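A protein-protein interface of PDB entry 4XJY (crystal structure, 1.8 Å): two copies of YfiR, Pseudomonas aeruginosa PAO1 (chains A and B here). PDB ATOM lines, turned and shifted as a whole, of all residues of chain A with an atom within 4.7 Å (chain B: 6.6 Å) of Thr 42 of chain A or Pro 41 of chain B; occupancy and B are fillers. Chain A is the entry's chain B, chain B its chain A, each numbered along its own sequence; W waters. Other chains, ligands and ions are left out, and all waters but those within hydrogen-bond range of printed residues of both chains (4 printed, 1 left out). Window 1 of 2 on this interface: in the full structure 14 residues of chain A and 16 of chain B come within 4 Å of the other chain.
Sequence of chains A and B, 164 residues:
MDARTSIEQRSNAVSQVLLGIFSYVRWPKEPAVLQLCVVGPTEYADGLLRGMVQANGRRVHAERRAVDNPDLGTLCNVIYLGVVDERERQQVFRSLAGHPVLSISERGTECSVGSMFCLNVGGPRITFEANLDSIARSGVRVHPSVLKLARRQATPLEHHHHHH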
ATOM      1  N   VAL A  38     -18.568 -23.395 -34.651  1.00  0.00           N
ATOM      2  CA  VAL A  38     -18.928 -23.524 -33.256  1.00  0.00           C
ATOM      3  C   VAL A  38     -20.297 -22.881 -33.192  1.00  0.00           C
ATOM      4  O   VAL A  38     -20.432 -21.709 -33.555  1.00  0.00           O
ATOM      5  CB  VAL A  38     -17.900 -22.785 -32.333  1.00  0.00           C
ATOM      6  CG1 VAL A  38     -18.326 -22.799 -30.852  1.00  0.00           C
ATOM      7  CG2 VAL A  38     -16.514 -23.417 -32.518  1.00  0.00           C
ATOM      8  N   GLY A  40     -23.865 -22.164 -30.966  1.00  0.00           N
ATOM      9  CA  GLY A  40     -24.522 -22.126 -29.669  1.00  0.00           C
ATOM     10  C   GLY A  40     -23.509 -21.807 -28.568  1.00  0.00           C
ATOM     11  O   GLY A  40     -22.279 -21.831 -28.803  1.00  0.00           O
ATOM     12  N   PRO A  41     -24.002 -21.578 -27.342  1.00  0.00           N
ATOM     13  CA  PRO A  41     -23.174 -21.246 -26.179  1.00  0.00           C
ATOM     14  C   PRO A  41     -22.227 -22.382 -25.832  1.00  0.00           C
ATOM     15  O   PRO A  41     -22.643 -23.546 -25.814  1.00  0.00           O
ATOM     16  CB  PRO A  41     -24.197 -21.017 -25.061  1.00  0.00           C
ATOM     17  CG  PRO A  41     -25.534 -20.770 -25.779  1.00  0.00           C
ATOM     18  CD  PRO A  41     -25.443 -21.569 -27.034  1.00  0.00           C
ATOM     19  N   THR A  42     -20.949 -22.063 -25.646  1.00  0.00           N
ATOM     20  CA  THR A  42     -19.955 -23.096 -25.343  1.00  0.00           C
ATOM     21  C   THR A  42     -19.063 -22.602 -24.236  1.00  0.00           C
ATOM     22  O   THR A  42     -18.819 -21.398 -24.111  1.00  0.00           O
ATOM     23  CB  THR A  42     -19.064 -23.459 -26.574  1.00  0.00           C
ATOM     24  OG1 THR A  42     -18.410 -22.269 -27.066  1.00  0.00           O
ATOM     25  CG2 THR A  42     -19.928 -24.092 -27.703  1.00  0.00           C
ATOM     26  N   GLU A  43     -18.537 -23.534 -23.459  1.00  0.00           N
ATOM     27  CA  GLU A  43     -17.619 -23.216 -22.376  1.00  0.00           C
ATOM     28  C   GLU A  43     -16.178 -23.589 -22.712  1.00  0.00           C
ATOM     29  O   GLU A  43     -15.245 -22.975 -22.187  1.00  0.00           O
ATOM     30  CB  GLU A  43     -18.051 -23.949 -21.121  1.00  0.00           C
ATOM     31  CG  GLU A  43     -17.348 -23.535 -19.867  1.00  0.00           C
ATOM     32  CD  GLU A  43     -18.089 -23.995 -18.627  1.00  0.00           C
ATOM     33  OE1 GLU A  43     -19.042 -24.806 -18.768  1.00  0.00           O
ATOM     34  OE2 GLU A  43     -17.712 -23.545 -17.525  1.00  0.00           O
ATOM     35  N   TYR A  44     -16.003 -24.617 -23.557  1.00  0.00           N
ATOM     36  CA  TYR A  44     -14.691 -25.243 -23.744  1.00  0.00           C
ATOM     37  C   TYR A  44     -14.126 -25.066 -25.154  1.00  0.00           C
ATOM     38  O   TYR A  44     -13.168 -25.756 -25.539  1.00  0.00           O
ATOM     39  CB  TYR A  44     -14.789 -26.747 -23.402  1.00  0.00           C
ATOM     40  CG  TYR A  44     -15.199 -26.989 -21.972  1.00  0.00           C
ATOM     41  CD1 TYR A  44     -14.363 -26.602 -20.936  1.00  0.00           C
ATOM     42  CD2 TYR A  44     -16.460 -27.501 -21.649  1.00  0.00           C
ATOM     43  CE1 TYR A  44     -14.725 -26.777 -19.616  1.00  0.00           C
ATOM     44  CE2 TYR A  44     -16.843 -27.681 -20.312  1.00  0.00           C
ATOM     45  CZ  TYR A  44     -15.964 -27.320 -19.311  1.00  0.00           C
ATOM     46  OH  TYR A  44     -16.284 -27.488 -17.980  1.00  0.00           O
ATOM     47  N   ALA A  45     -14.656 -24.109 -25.916  1.00  0.00           N
ATOM     48  CA  ALA A  45     -14.214 -23.964 -27.304  1.00  0.00           C
ATOM     49  C   ALA A  45     -13.156 -22.858 -27.516  1.00  0.00           C
ATOM     50  O   ALA A  45     -12.761 -22.605 -28.649  1.00  0.00           O
ATOM     51  CB  ALA A  45     -15.425 -23.717 -28.228  1.00  0.00           C
ATOM     52  N   ARG A  64     -17.397 -19.028 -35.049  1.00  0.00           N
ATOM     53  CA  ARG A  64     -18.703 -19.209 -34.451  1.00  0.00           C
ATOM     54  C   ARG A  64     -19.767 -18.867 -35.476  1.00  0.00           C
ATOM     55  O   ARG A  64     -19.620 -17.878 -36.194  1.00  0.00           O
ATOM     56  CB  ARG A  64     -18.887 -18.305 -33.214  1.00  0.00           C
ATOM     57  CG  ARG A  64     -18.096 -18.779 -31.981  1.00  0.00           C
ATOM     58  CD  ARG A  64     -18.509 -17.918 -30.751  1.00  0.00           C
ATOM     59  NE  ARG A  64     -17.551 -18.079 -29.679  1.00  0.00           N
ATOM     60  CZ  ARG A  64     -17.655 -18.992 -28.720  1.00  0.00           C
ATOM     61  NH1 ARG A  64     -18.695 -19.810 -28.715  1.00  0.00           N
ATOM     62  NH2 ARG A  64     -16.713 -19.085 -27.773  1.00  0.00           N
ATOM     63  N   TYR A  80     -19.276 -28.047 -33.945  1.00  0.00           N
ATOM     64  CA  TYR A  80     -19.107 -28.244 -32.511  1.00  0.00           C
ATOM     65  C   TYR A  80     -20.302 -27.574 -31.891  1.00  0.00           C
ATOM     66  O   TYR A  80     -20.412 -26.349 -31.928  1.00  0.00           O
ATOM     67  CB  TYR A  80     -17.804 -27.612 -32.013  1.00  0.00           C
ATOM     68  CG  TYR A  80     -17.522 -27.815 -30.549  1.00  0.00           C
ATOM     69  CD1 TYR A  80     -16.950 -29.004 -30.085  1.00  0.00           C
ATOM     70  CD2 TYR A  80     -17.797 -26.805 -29.622  1.00  0.00           C
ATOM     71  CE1 TYR A  80     -16.664 -29.192 -28.725  1.00  0.00           C
ATOM     72  CE2 TYR A  80     -17.502 -26.969 -28.265  1.00  0.00           C
ATOM     73  CZ  TYR A  80     -16.931 -28.144 -27.826  1.00  0.00           C
ATOM     74  OH  TYR A  80     -16.679 -28.311 -26.500  1.00  0.00           O
ATOM     75  N   GLY A  82     -22.956 -26.326 -29.143  1.00  0.00           N
ATOM     76  CA  GLY A  82     -23.124 -25.902 -27.761  1.00  0.00           C
ATOM     77  C   GLY A  82     -24.548 -26.114 -27.264  1.00  0.00           C
ATOM     78  O   GLY A  82     -25.282 -27.004 -27.720  1.00  0.00           O
ATOM     79  N   VAL A  83     -24.970 -25.277 -26.319  1.00  0.00           N
ATOM     80  CA  VAL A  83     -26.290 -25.432 -25.719  1.00  0.00           C
ATOM     81  C   VAL A  83     -27.415 -25.019 -26.655  1.00  0.00           C
ATOM     82  O   VAL A  83     -27.477 -23.878 -27.101  1.00  0.00           O
ATOM     83  CB  VAL A  83     -26.434 -24.598 -24.427  1.00  0.00           C
ATOM     84  CG1 VAL A  83     -27.841 -24.742 -23.850  1.00  0.00           C
ATOM     85  CG2 VAL A  83     -25.355 -24.977 -23.423  1.00  0.00           C
ATOM     86  N   GLU A 106     -20.797 -30.498 -27.118  1.00  0.00           N
ATOM     87  CA  GLU A 106     -19.970 -30.248 -25.945  1.00  0.00           C
ATOM     88  C   GLU A 106     -20.534 -30.919 -24.683  1.00  0.00           C
ATOM     89  O   GLU A 106     -19.778 -31.406 -23.834  1.00  0.00           O
ATOM     90  CB  GLU A 106     -19.862 -28.736 -25.704  1.00  0.00           C
ATOM     91  CG  GLU A 106     -19.169 -28.370 -24.390  1.00  0.00           C
ATOM     92  CD  GLU A 106     -18.828 -26.887 -24.291  1.00  0.00           C
ATOM     93  OE1 GLU A 106     -17.851 -26.476 -24.952  1.00  0.00           O
ATOM     94  OE2 GLU A 106     -19.557 -26.141 -23.576  1.00  0.00           O
ATOM     95  N   ARG A 107     -21.857 -30.816 -24.530  1.00  0.00           N
ATOM     96  CA  ARG A 107     -22.571 -31.316 -23.350  1.00  0.00           C
ATOM     97  C   ARG A 107     -23.991 -31.786 -23.662  1.00  0.00           C
ATOM     98  O   ARG A 107     -24.592 -31.393 -24.676  1.00  0.00           O
ATOM     99  CB  ARG A 107     -22.608 -30.242 -22.234  1.00  0.00           C
ATOM    100  CG  ARG A 107     -23.695 -29.158 -22.348  1.00  0.00           C
ATOM    101  CD  ARG A 107     -23.530 -28.049 -21.256  1.00  0.00           C
ATOM    102  NE  ARG A 107     -22.219 -27.425 -21.385  1.00  0.00           N
ATOM    103  CZ  ARG A 107     -21.546 -26.812 -20.412  1.00  0.00           C
ATOM    104  NH1 ARG A 107     -22.049 -26.685 -19.174  1.00  0.00           N
ATOM    105  NH2 ARG A 107     -20.352 -26.313 -20.693  1.00  0.00           N
ATOM    106  N   VAL B  38     -15.813 -14.631 -17.065  1.00  0.00           N
ATOM    107  CA  VAL B  38     -16.821 -15.246 -17.902  1.00  0.00           C
ATOM    108  C   VAL B  38     -17.060 -16.650 -17.357  1.00  0.00           C
ATOM    109  O   VAL B  38     -16.126 -17.433 -17.203  1.00  0.00           O
ATOM    110  CB  VAL B  38     -16.394 -15.277 -19.377  1.00  0.00           C
ATOM    111  CG1 VAL B  38     -17.466 -16.031 -20.268  1.00  0.00           C
ATOM    112  CG2 VAL B  38     -16.213 -13.863 -19.863  1.00  0.00           C
ATOM    113  N   VAL B  39     -18.316 -16.975 -17.046  1.00  0.00           N
ATOM    114  CA  VAL B  39     -18.575 -18.226 -16.357  1.00  0.00           C
ATOM    115  C   VAL B  39     -19.698 -18.985 -17.057  1.00  0.00           C
ATOM    116  O   VAL B  39     -20.812 -18.471 -17.193  1.00  0.00           O
ATOM    117  CB  VAL B  39     -18.896 -17.967 -14.861  1.00  0.00           C
ATOM    118  CG1 VAL B  39     -19.274 -19.244 -14.101  1.00  0.00           C
ATOM    119  CG2 VAL B  39     -17.675 -17.298 -14.183  1.00  0.00           C
ATOM    120  N   GLY B  40     -19.383 -20.187 -17.534  1.00  0.00           N
ATOM    121  CA  GLY B  40     -20.385 -21.026 -18.186  1.00  0.00           C
ATOM    122  C   GLY B  40     -20.434 -20.857 -19.694  1.00  0.00           C
ATOM    123  O   GLY B  40     -19.732 -20.032 -20.270  1.00  0.00           O
ATOM    124  N   PRO B  41     -21.269 -21.662 -20.366  1.00  0.00           N
ATOM    125  CA  PRO B  41     -21.340 -21.562 -21.829  1.00  0.00           C
ATOM    126  C   PRO B  41     -21.843 -20.228 -22.346  1.00  0.00           C
ATOM    127  O   PRO B  41     -22.898 -19.756 -21.932  1.00  0.00           O
ATOM    128  CB  PRO B  41     -22.351 -22.657 -22.217  1.00  0.00           C
ATOM    129  CG  PRO B  41     -22.432 -23.579 -21.030  1.00  0.00           C
ATOM    130  CD  PRO B  41     -22.150 -22.708 -19.824  1.00  0.00           C
ATOM    131  N   THR B  42     -21.123 -19.661 -23.300  1.00  0.00           N
ATOM    132  CA  THR B  42     -21.485 -18.397 -23.893  1.00  0.00           C
ATOM    133  C   THR B  42     -21.283 -18.392 -25.398  1.00  0.00           C
ATOM    134  O   THR B  42     -20.420 -19.125 -25.948  1.00  0.00           O
ATOM    135  CB  THR B  42     -20.645 -17.228 -23.285  1.00  0.00           C
ATOM    136  OG1 THR B  42     -19.262 -17.577 -23.369  1.00  0.00           O
ATOM    137  CG2 THR B  42     -20.973 -16.983 -21.786  1.00  0.00           C
ATOM    138  N   GLU B  43     -22.017 -17.529 -26.077  1.00  0.00           N
ATOM    139  CA  GLU B  43     -21.846 -17.341 -27.526  1.00  0.00           C
ATOM    140  C   GLU B  43     -21.119 -16.051 -27.851  1.00  0.00           C
ATOM    141  O   GLU B  43     -20.508 -15.935 -28.904  1.00  0.00           O
ATOM    142  CB  GLU B  43     -23.197 -17.266 -28.269  1.00  0.00           C
ATOM    143  CG  GLU B  43     -23.928 -18.502 -28.402  1.00  0.00           C
ATOM    144  CD  GLU B  43     -25.166 -18.330 -29.243  1.00  0.00           C
ATOM    145  OE1 GLU B  43     -26.190 -18.005 -28.635  1.00  0.00           O
ATOM    146  OE2 GLU B  43     -25.100 -18.497 -30.484  1.00  0.00           O
ATOM    147  N   ARG B  64     -11.836 -16.582 -18.265  1.00  0.00           N
ATOM    148  CA  ARG B  64     -12.921 -17.550 -18.135  1.00  0.00           C
ATOM    149  C   ARG B  64     -12.672 -18.396 -16.872  1.00  0.00           C
ATOM    150  O   ARG B  64     -11.563 -18.937 -16.685  1.00  0.00           O
ATOM    151  CB  ARG B  64     -12.995 -18.409 -19.395  1.00  0.00           C
ATOM    152  CG  ARG B  64     -14.008 -19.500 -19.284  1.00  0.00           C
ATOM    153  CD  ARG B  64     -14.135 -20.288 -20.581  1.00  0.00           C
ATOM    154  NE  ARG B  64     -14.851 -19.576 -21.642  1.00  0.00           N
ATOM    155  CZ  ARG B  64     -16.164 -19.366 -21.599  1.00  0.00           C
ATOM    156  NH1 ARG B  64     -16.851 -19.717 -20.509  1.00  0.00           N
ATOM    157  NH2 ARG B  64     -16.773 -18.752 -22.602  1.00  0.00           N
ATOM    158  N   VAL B  67     -17.731 -22.561 -12.966  1.00  0.00           N
ATOM    159  CA  VAL B  67     -18.925 -22.383 -12.157  1.00  0.00           C
ATOM    160  C   VAL B  67     -18.681 -22.749 -10.708  1.00  0.00           C
ATOM    161  O   VAL B  67     -19.210 -22.088  -9.802  1.00  0.00           O
ATOM    162  CB  VAL B  67     -20.077 -23.258 -12.701  1.00  0.00           C
ATOM    163  CG1 VAL B  67     -21.196 -23.396 -11.643  1.00  0.00           C
ATOM    164  CG2 VAL B  67     -20.600 -22.649 -13.991  1.00  0.00           C
ATOM    165  N   LEU B  81     -22.334 -14.178 -16.999  1.00  0.00           N
ATOM    166  CA  LEU B  81     -22.810 -15.521 -16.718  1.00  0.00           C
ATOM    167  C   LEU B  81     -23.481 -16.124 -17.946  1.00  0.00           C
ATOM    168  O   LEU B  81     -24.414 -15.550 -18.504  1.00  0.00           O
ATOM    169  CB  LEU B  81     -23.783 -15.489 -15.531  1.00  0.00           C
ATOM    170  CG  LEU B  81     -24.237 -16.855 -14.997  1.00  0.00           C
ATOM    171  CD1 LEU B  81     -23.027 -17.642 -14.465  1.00  0.00           C
ATOM    172  CD2 LEU B  81     -25.331 -16.697 -13.910  1.00  0.00           C
ATOM    173  N   GLY B  82     -22.998 -17.287 -18.376  1.00  0.00           N
ATOM    174  CA  GLY B  82     -23.571 -17.900 -19.536  1.00  0.00           C
ATOM    175  C   GLY B  82     -24.734 -18.780 -19.206  1.00  0.00           C
ATOM    176  O   GLY B  82     -25.401 -18.621 -18.172  1.00  0.00           O
ATOM    177  N   VAL B  83     -24.997 -19.690 -20.130  1.00  0.00           N
ATOM    178  CA  VAL B  83     -26.177 -20.525 -20.058  1.00  0.00           C
ATOM    179  C   VAL B  83     -25.930 -21.734 -19.190  1.00  0.00           C
ATOM    180  O   VAL B  83     -25.708 -22.820 -19.727  1.00  0.00           O
ATOM    181  CB  VAL B  83     -26.581 -20.960 -21.481  1.00  0.00           C
ATOM    182  CG1 VAL B  83     -27.930 -21.689 -21.482  1.00  0.00           C
ATOM    183  CG2 VAL B  83     -26.652 -19.730 -22.379  1.00  0.00           C
ATOM    184  N   VAL B  84     -26.226 -21.598 -17.903  1.00  0.00           N
ATOM    185  CA  VAL B  84     -26.004 -22.640 -16.904  1.00  0.00           C
ATOM    186  C   VAL B  84     -27.355 -23.121 -16.372  1.00  0.00           C
ATOM    187  O   VAL B  84     -28.358 -22.401 -16.478  1.00  0.00           O
ATOM    188  CB  VAL B  84     -25.166 -22.124 -15.717  1.00  0.00           C
ATOM    189  CG1 VAL B  84     -23.782 -21.696 -16.215  1.00  0.00           C
ATOM    190  CG2 VAL B  84     -25.872 -20.941 -15.044  1.00  0.00           C
ATOM    191  N   GLU B  88     -26.273 -24.873 -11.130  1.00  0.00           N
ATOM    192  CA  GLU B  88     -25.040 -24.141 -11.395  1.00  0.00           C
ATOM    193  C   GLU B  88     -25.226 -22.682 -11.038  1.00  0.00           C
ATOM    194  O   GLU B  88     -24.319 -22.052 -10.446  1.00  0.00           O
ATOM    195  CB  GLU B  88     -24.630 -24.304 -12.853  1.00  0.00           C
ATOM    196  CG  GLU B  88     -24.238 -25.736 -13.187  1.00  0.00           C
ATOM    197  CD  GLU B  88     -24.046 -25.953 -14.668  1.00  0.00           C
ATOM    198  OE1 GLU B  88     -24.792 -25.335 -15.459  1.00  0.00           O
ATOM    199  OE2 GLU B  88     -23.169 -26.762 -15.046  1.00  0.00           O
ATOM    200  N   GLU B 106     -25.885 -13.524 -20.176  1.00  0.00           N
ATOM    201  CA  GLU B 106     -25.912 -13.396 -21.613  1.00  0.00           C
ATOM    202  C   GLU B 106     -27.359 -13.471 -22.117  1.00  0.00           C
ATOM    203  O   GLU B 106     -27.707 -12.814 -23.093  1.00  0.00           O
ATOM    204  CB  GLU B 106     -25.075 -14.480 -22.266  1.00  0.00           C
ATOM    205  CG  GLU B 106     -25.173 -14.484 -23.782  1.00  0.00           C
ATOM    206  CD  GLU B 106     -24.026 -15.274 -24.410  1.00  0.00           C
ATOM    207  OE1 GLU B 106     -22.898 -14.754 -24.443  1.00  0.00           O
ATOM    208  OE2 GLU B 106     -24.249 -16.415 -24.877  1.00  0.00           O
HETATM  209  O   HOH W   1     -15.605 -17.667 -25.148  1.00  0.00           O
HETATM  210  O   HOH W   2     -18.477 -16.908 -26.054  1.00  0.00           O
HETATM  211  O   HOH W   3     -16.535 -20.972 -17.830  1.00  0.00           O
HETATM  212  O   HOH W   4     -22.981 -19.519 -32.036  1.00  0.00           O
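The guanidinium group (NE) of Arg 64 of chain B sits close to the backbone carbonyl oxygen (O) of Glu 43 of chain A (3.5 Å). N of Thr 42 of chain B is in hydrogen-bond range of O of Thr 42 of chain A, at 3.0 Å. The guanidinium group (NH1) of Arg 64 of chain A is in hydrogen-bond range of the backbone carbonyl oxygen (O) of Thr 42 of chain B (3.3 Å).
The backbone carbonyl oxygen (O) of Pro 41 of chain A sits at hydrogen-bond distance from the backbone NH (N) of Val 83 of chain A, at 2.9 Å. The side-chain carboxylate (OE2) of Glu 106 of chain A is in salt-bridge range of the guanidinium group (NH2) of Arg 107 of chain A. OE2 of Glu 106 of chain A sits at hydrogen-bond distance from N of Glu 43 of chain A (2.8 Å). The side-chain hydroxyl (OG1) of Thr 42 of chain B is in hydrogen-bond range of the guanidinium group (NH2) of Arg 64 of chain B (2.9 Å). NH1 of Arg 64 of chain B lies within hydrogen-bond range of O of Gly 40 of chain B (2.9 Å). The guanidinium group of Arg 107 of chain A is in salt-bridge range of the side-chain carboxylate of Glu 43 of chain A, 2.8 Å away.
Gly 40 of chain A touches Glu 43 of chain B. CA of Pro 41 of chain A touches O of Thr 42 of chain B (3.5 Å). Pro 41 of chain A touches Glu 43 of chain B. CG2 of Val 83 of chain B touches CG of Pro 41 of chain A, 3.7 Å away. Thr 42 of chain A touches Pro 41 of chain B. Glu 43 of chain A touches Gly 40 of chain B. N of Glu 43 of chain A touches CA of Pro 41 of chain B, at 3.8 Å. Arg 64 of chain A touches Glu 43 of chain B. CG1 of Val 83 of chain A touches CG1 of Val 83 of chain B (3.9 Å). Pro 41 of chain B touches Arg 107 of chain A.
Of the printed residues of chain A, Pro 41 of chain B touches Pro 41 (3.6 Å), Thr 42 (3.4 Å), Glu 43 (3.8 Å), Val 83 (3.98 Å) and Arg 107 (3.4 Å). Of the printed residues of chain A, Glu 43 of chain B touches Gly 40 (3.3 Å), Pro 41 (3.3 Å) and Arg 64 (3.4 Å). Of the printed residues of chain B, Glu 43 of chain A touches Gly 40, Pro 41 and Arg 64. Of the printed residues of chain B, Arg 64 of chain A touches Thr 42 and Glu 43. Leu 81 of chain B touches none of the printed residues of chain A.
Of the 14 printed residues of chain B, 6 touch a printed residue of chain A. Printed residues of chain B that touch a printed residue of chain A: Gly 40, Pro 41, Thr 42, Glu 43, Arg 64 and Val 83. Hydrophobic or aromatic side chains of chain B within 4 Å of the printed part of chain A: Pro 41 and Val 83. Along chain B the printed residues that touch a printed residue of chain A span positions 40 to 83. Hydrophobic or aromatic side chains of chain A that line the printed part of chain B: Pro 41 and Val 83. Among the printed residues, 16 pairs touch across the chains.
Pro 41 of chain B touches its own counterpart, Pro 41 of chain A. Pro 41 of chain A touches Thr 42 of chain B, and with the chains exchanged Thr 42 of chain A touches Pro 41 of chain B. Pro 41 of chain A touches Val 83 of chain B, and with the chains exchanged Val 83 of chain A touches Pro 41 of chain B. Val 83 of chain B touches its own counterpart, Val 83 of chain A. 9 positions are printed for both chains.
Water W4 bridges OE2 of Glu 43 of chain B (2.8 Å) and N of Gly 40 of chain A (3.0 Å). Water W3 lies within hydrogen-bond range of the side-chain carboxylate of Glu 43 of chain A (2.8 Å), the backbone NH of Gly 40 of chain B (3.0 Å) and the guanidinium group of Arg 64 of chain B (3.0 Å). Water W2 lies within hydrogen-bond range of OG1 of Thr 42 of chain B and NH2 of Arg 64 of chain A. Water W1 bridges the guanidinium group (NH2) of Arg 64 of chain B (3.0 Å) and the guanidinium group (NH2) of Arg 64 of chain A (3.2 Å).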
